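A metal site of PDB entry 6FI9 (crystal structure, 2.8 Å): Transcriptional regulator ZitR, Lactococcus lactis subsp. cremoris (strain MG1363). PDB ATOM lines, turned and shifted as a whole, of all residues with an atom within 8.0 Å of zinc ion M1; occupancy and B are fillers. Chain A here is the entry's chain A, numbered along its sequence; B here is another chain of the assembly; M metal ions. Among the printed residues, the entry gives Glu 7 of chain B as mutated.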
ATOM      1  N   GLU A  22       3.307 -12.516  18.208  1.00  0.00           N
ATOM      2  CA  GLU A  22       2.457 -12.020  19.288  1.00  0.00           C
ATOM      3  C   GLU A  22       2.750 -10.560  19.618  1.00  0.00           C
ATOM      4  O   GLU A  22       3.872 -10.086  19.402  1.00  0.00           O
ATOM      5  CB  GLU A  22       2.599 -12.888  20.559  1.00  0.00           C
ATOM      6  CG  GLU A  22       4.007 -12.976  21.129  1.00  0.00           C
ATOM      7  CD  GLU A  22       4.147 -13.969  22.266  1.00  0.00           C
ATOM      8  OE1 GLU A  22       3.386 -13.865  23.255  1.00  0.00           O
ATOM      9  OE2 GLU A  22       5.016 -14.866  22.171  1.00  0.00           O
ATOM     10  N   ILE A  23       1.746  -9.845  20.130  1.00  0.00           N
ATOM     11  CA  ILE A  23       1.886  -8.455  20.516  1.00  0.00           C
ATOM     12  C   ILE A  23       2.223  -8.346  22.011  1.00  0.00           C
ATOM     13  O   ILE A  23       1.458  -8.787  22.869  1.00  0.00           O
ATOM     14  CB  ILE A  23       0.653  -7.583  20.092  1.00  0.00           C
ATOM     15  CG1 ILE A  23       0.626  -7.392  18.573  1.00  0.00           C
ATOM     16  CG2 ILE A  23       0.654  -6.229  20.811  1.00  0.00           C
ATOM     17  CD1 ILE A  23      -0.695  -6.974  18.054  1.00  0.00           C
ATOM     18  N   LEU A  24       3.395  -7.761  22.301  1.00  0.00           N
ATOM     19  CA  LEU A  24       3.882  -7.525  23.655  1.00  0.00           C
ATOM     20  C   LEU A  24       4.358  -6.093  23.732  1.00  0.00           C
ATOM     21  O   LEU A  24       5.301  -5.722  23.037  1.00  0.00           O
ATOM     22  CB  LEU A  24       5.018  -8.495  24.018  1.00  0.00           C
ATOM     23  CG  LEU A  24       4.598  -9.914  24.426  1.00  0.00           C
ATOM     24  CD1 LEU A  24       5.656 -10.917  24.015  1.00  0.00           C
ATOM     25  CD2 LEU A  24       4.331 -10.011  25.907  1.00  0.00           C
ATOM     26  N   THR A  35      13.675 -15.520  20.719  1.00  0.00           N
ATOM     27  CA  THR A  35      12.563 -14.910  19.983  1.00  0.00           C
ATOM     28  C   THR A  35      11.266 -14.888  20.806  1.00  0.00           C
ATOM     29  O   THR A  35      11.229 -15.425  21.917  1.00  0.00           O
ATOM     30  CB  THR A  35      12.363 -15.563  18.598  1.00  0.00           C
ATOM     31  OG1 THR A  35      12.149 -16.970  18.748  1.00  0.00           O
ATOM     32  CG2 THR A  35      13.515 -15.297  17.641  1.00  0.00           C
ATOM     33  N   SER A  36      10.203 -14.261  20.248  1.00  0.00           N
ATOM     34  CA  SER A  36       8.879 -14.139  20.876  1.00  0.00           C
ATOM     35  C   SER A  36       8.310 -15.514  21.245  1.00  0.00           C
ATOM     36  O   SER A  36       7.993 -15.754  22.414  1.00  0.00           O
ATOM     37  CB  SER A  36       7.917 -13.380  19.954  1.00  0.00           C
ATOM     38  OG  SER A  36       8.398 -12.090  19.604  1.00  0.00           O
ATOM     39  N   THR A  37       8.236 -16.421  20.246  1.00  0.00           N
ATOM     40  CA  THR A  37       7.718 -17.786  20.391  1.00  0.00           C
ATOM     41  C   THR A  37       8.562 -18.632  21.337  1.00  0.00           C
ATOM     42  O   THR A  37       8.005 -19.295  22.215  1.00  0.00           O
ATOM     43  CB  THR A  37       7.527 -18.452  19.018  1.00  0.00           C
ATOM     44  OG1 THR A  37       8.769 -18.432  18.309  1.00  0.00           O
ATOM     45  CG2 THR A  37       6.434 -17.798  18.179  1.00  0.00           C
ATOM     46  N   GLN A  38       9.905 -18.589  21.161  1.00  0.00           N
ATOM     47  CA  GLN A  38      10.878 -19.333  21.969  1.00  0.00           C
ATOM     48  C   GLN A  38      10.711 -19.100  23.473  1.00  0.00           C
ATOM     49  O   GLN A  38      10.722 -20.066  24.250  1.00  0.00           O
ATOM     50  CB  GLN A  38      12.315 -19.025  21.528  1.00  0.00           C
ATOM     51  CG  GLN A  38      12.772 -19.854  20.338  1.00  0.00           C
ATOM     52  CD  GLN A  38      14.172 -19.472  19.911  1.00  0.00           C
ATOM     53  OE1 GLN A  38      14.405 -18.392  19.361  1.00  0.00           O
ATOM     54  NE2 GLN A  38      15.123 -20.357  20.154  1.00  0.00           N
ATOM     55  N   GLU A  39      10.542 -17.820  23.882  1.00  0.00           N
ATOM     56  CA  GLU A  39      10.348 -17.456  25.285  1.00  0.00           C
ATOM     57  C   GLU A  39       8.986 -17.909  25.789  1.00  0.00           C
ATOM     58  O   GLU A  39       8.871 -18.357  26.931  1.00  0.00           O
ATOM     59  CB  GLU A  39      10.549 -15.954  25.491  1.00  0.00           C
ATOM     60  CG  GLU A  39      12.006 -15.585  25.729  1.00  0.00           C
ATOM     61  CD  GLU A  39      12.291 -14.137  26.069  1.00  0.00           C
ATOM     62  OE1 GLU A  39      11.567 -13.563  26.912  1.00  0.00           O
ATOM     63  OE2 GLU A  39      13.263 -13.574  25.498  1.00  0.00           O
ATOM     64  N   HIS A  40       7.976 -17.839  24.913  1.00  0.00           N
ATOM     65  CA  HIS A  40       6.608 -18.259  25.232  1.00  0.00           C
ATOM     66  C   HIS A  40       6.510 -19.775  25.440  1.00  0.00           C
ATOM     67  O   HIS A  40       5.740 -20.209  26.292  1.00  0.00           O
ATOM     68  CB  HIS A  40       5.603 -17.755  24.192  1.00  0.00           C
ATOM     69  CG  HIS A  40       4.178 -17.994  24.584  1.00  0.00           C
ATOM     70  ND1 HIS A  40       3.594 -17.277  25.614  1.00  0.00           N
ATOM     71  CD2 HIS A  40       3.282 -18.885  24.105  1.00  0.00           C
ATOM     72  CE1 HIS A  40       2.362 -17.755  25.717  1.00  0.00           C
ATOM     73  NE2 HIS A  40       2.127 -18.720  24.829  1.00  0.00           N
ATOM     74  N   ILE A  41       7.315 -20.569  24.688  1.00  0.00           N
ATOM     75  CA  ILE A  41       7.353 -22.022  24.829  1.00  0.00           C
ATOM     76  C   ILE A  41       7.797 -22.367  26.267  1.00  0.00           C
ATOM     77  O   ILE A  41       7.206 -23.235  26.903  1.00  0.00           O
ATOM     78  CB  ILE A  41       8.216 -22.693  23.720  1.00  0.00           C
ATOM     79  CG1 ILE A  41       7.543 -22.550  22.342  1.00  0.00           C
ATOM     80  CG2 ILE A  41       8.491 -24.167  24.016  1.00  0.00           C
ATOM     81  CD1 ILE A  41       8.494 -22.527  21.125  1.00  0.00           C
ATOM     82  N   MET A  43       7.430 -20.442  28.925  1.00  0.00           N
ATOM     83  CA  MET A  43       6.359 -19.958  29.793  1.00  0.00           C
ATOM     84  C   MET A  43       5.273 -21.029  30.029  1.00  0.00           C
ATOM     85  O   MET A  43       4.932 -21.282  31.182  1.00  0.00           O
ATOM     86  CB  MET A  43       5.765 -18.662  29.216  1.00  0.00           C
ATOM     87  CG  MET A  43       4.753 -17.995  30.103  1.00  0.00           C
ATOM     88  SD  MET A  43       3.922 -16.659  29.234  1.00  0.00           S
ATOM     89  CE  MET A  43       2.418 -16.594  30.168  1.00  0.00           C
ATOM     90  N   ILE A  44       4.764 -21.656  28.942  1.00  0.00           N
ATOM     91  CA  ILE A  44       3.727 -22.707  29.002  1.00  0.00           C
ATOM     92  C   ILE A  44       4.266 -24.024  29.580  1.00  0.00           C
ATOM     93  O   ILE A  44       3.507 -24.773  30.179  1.00  0.00           O
ATOM     94  CB  ILE A  44       2.968 -22.932  27.650  1.00  0.00           C
ATOM     95  CG1 ILE A  44       3.933 -23.265  26.483  1.00  0.00           C
ATOM     96  CG2 ILE A  44       2.061 -21.748  27.329  1.00  0.00           C
ATOM     97  CD1 ILE A  44       3.372 -24.242  25.471  1.00  0.00           C
ATOM     98  N   LEU A  59       0.465 -22.559  21.103  1.00  0.00           N
ATOM     99  CA  LEU A  59       1.060 -21.461  20.338  1.00  0.00           C
ATOM    100  C   LEU A  59       0.350 -21.156  19.028  1.00  0.00           C
ATOM    101  O   LEU A  59       0.562 -20.076  18.460  1.00  0.00           O
ATOM    102  CB  LEU A  59       2.547 -21.736  20.081  1.00  0.00           C
ATOM    103  CG  LEU A  59       3.520 -21.206  21.120  1.00  0.00           C
ATOM    104  CD1 LEU A  59       3.759 -22.220  22.223  1.00  0.00           C
ATOM    105  CD2 LEU A  59       4.835 -20.839  20.459  1.00  0.00           C
ATOM    106  N   HIS A 106       8.648 -13.647  30.881  1.00  0.00           N
ATOM    107  CA  HIS A 106       7.651 -13.628  29.806  1.00  0.00           C
ATOM    108  C   HIS A 106       6.240 -13.541  30.375  1.00  0.00           C
ATOM    109  O   HIS A 106       5.423 -12.798  29.848  1.00  0.00           O
ATOM    110  CB  HIS A 106       7.806 -14.836  28.893  1.00  0.00           C
ATOM    111  CG  HIS A 106       7.304 -14.590  27.504  1.00  0.00           C
ATOM    112  ND1 HIS A 106       8.016 -13.821  26.613  1.00  0.00           N
ATOM    113  CD2 HIS A 106       6.167 -15.024  26.910  1.00  0.00           C
ATOM    114  CE1 HIS A 106       7.295 -13.813  25.499  1.00  0.00           C
ATOM    115  NE2 HIS A 106       6.182 -14.521  25.633  1.00  0.00           N
ATOM    116  N   ALA A 107       5.974 -14.264  31.477  1.00  0.00           N
ATOM    117  CA  ALA A 107       4.690 -14.253  32.170  1.00  0.00           C
ATOM    118  C   ALA A 107       4.408 -12.860  32.756  1.00  0.00           C
ATOM    119  O   ALA A 107       3.267 -12.420  32.794  1.00  0.00           O
ATOM    120  CB  ALA A 107       4.692 -15.299  33.264  1.00  0.00           C
ATOM    121  N   HIS A 109       5.868 -10.088  31.376  1.00  0.00           N
ATOM    122  CA  HIS A 109       5.797  -9.280  30.152  1.00  0.00           C
ATOM    123  C   HIS A 109       4.393  -9.362  29.530  1.00  0.00           C
ATOM    124  O   HIS A 109       3.963  -8.406  28.882  1.00  0.00           O
ATOM    125  CB  HIS A 109       6.883  -9.717  29.151  1.00  0.00           C
ATOM    126  CG  HIS A 109       7.158  -8.750  28.037  1.00  0.00           C
ATOM    127  ND1 HIS A 109       7.908  -9.127  26.936  1.00  0.00           N
ATOM    128  CD2 HIS A 109       6.796  -7.454  27.894  1.00  0.00           C
ATOM    129  CE1 HIS A 109       7.970  -8.055  26.159  1.00  0.00           C
ATOM    130  NE2 HIS A 109       7.310  -7.023  26.695  1.00  0.00           N
ATOM    131  N   HIS A 110       3.683 -10.479  29.725  1.00  0.00           N
ATOM    132  CA  HIS A 110       2.313 -10.667  29.266  1.00  0.00           C
ATOM    133  C   HIS A 110       1.330  -9.911  30.151  1.00  0.00           C
ATOM    134  O   HIS A 110       0.396  -9.295  29.634  1.00  0.00           O
ATOM    135  CB  HIS A 110       1.949 -12.161  29.218  1.00  0.00           C
ATOM    136  CG  HIS A 110       2.088 -12.751  27.849  1.00  0.00           C
ATOM    137  ND1 HIS A 110       1.206 -12.414  26.825  1.00  0.00           N
ATOM    138  CD2 HIS A 110       2.991 -13.634  27.371  1.00  0.00           C
ATOM    139  CE1 HIS A 110       1.607 -13.109  25.774  1.00  0.00           C
ATOM    140  NE2 HIS A 110       2.686 -13.854  26.052  1.00  0.00           N
ATOM    141  N   GLU B   7      -6.643  -8.022  24.379  1.00  0.00           N
ATOM    142  CA  GLU B   7      -5.606  -9.025  24.108  1.00  0.00           C
ATOM    143  C   GLU B   7      -6.109 -10.025  23.056  1.00  0.00           C
ATOM    144  O   GLU B   7      -5.345 -10.401  22.175  1.00  0.00           O
ATOM    145  CB  GLU B   7      -5.204  -9.760  25.404  1.00  0.00           C
ATOM    146  CG  GLU B   7      -3.939 -10.609  25.244  1.00  0.00           C
ATOM    147  CD  GLU B   7      -3.476 -11.419  26.452  1.00  0.00           C
ATOM    148  OE1 GLU B   7      -4.273 -12.236  26.962  1.00  0.00           O
ATOM    149  OE2 GLU B   7      -2.302 -11.249  26.852  1.00  0.00           O
HETATM  150 ZN    ZN M   1       4.129 -14.599  24.953  1.00  0.00          ZN
HETATM  151 ZN    ZN M   2      10.532 -11.746  27.968  1.00  0.00          ZN
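ND1 of His 40 is in hydrogen-bond range of SD of Met 43 (3.7 Å).
Four residues have an atom within 4 Å of zinc ion M1: Glu 22, His 40, His 106 and His 110. Along chain A the residues within 4 Å of zinc ion M1 span positions 22 to 110. The nearest printed residue that does not touch zinc ion M1 is Leu 24 (4.1 Å).
Zinc ion M1 is bound by a ring nitrogen (NE2) of His 110 (2.0 Å), the side-chain carboxylate (OE1) of Glu 22 (2.0 Å) and a ring nitrogen (NE2) of His 106 (2.2 Å). Zinc ion M1 has three donor atoms within binding distance. Slightly farther from zinc ion M1 lies a ring nitrogen (ND1) of His 40 (2.8 Å).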
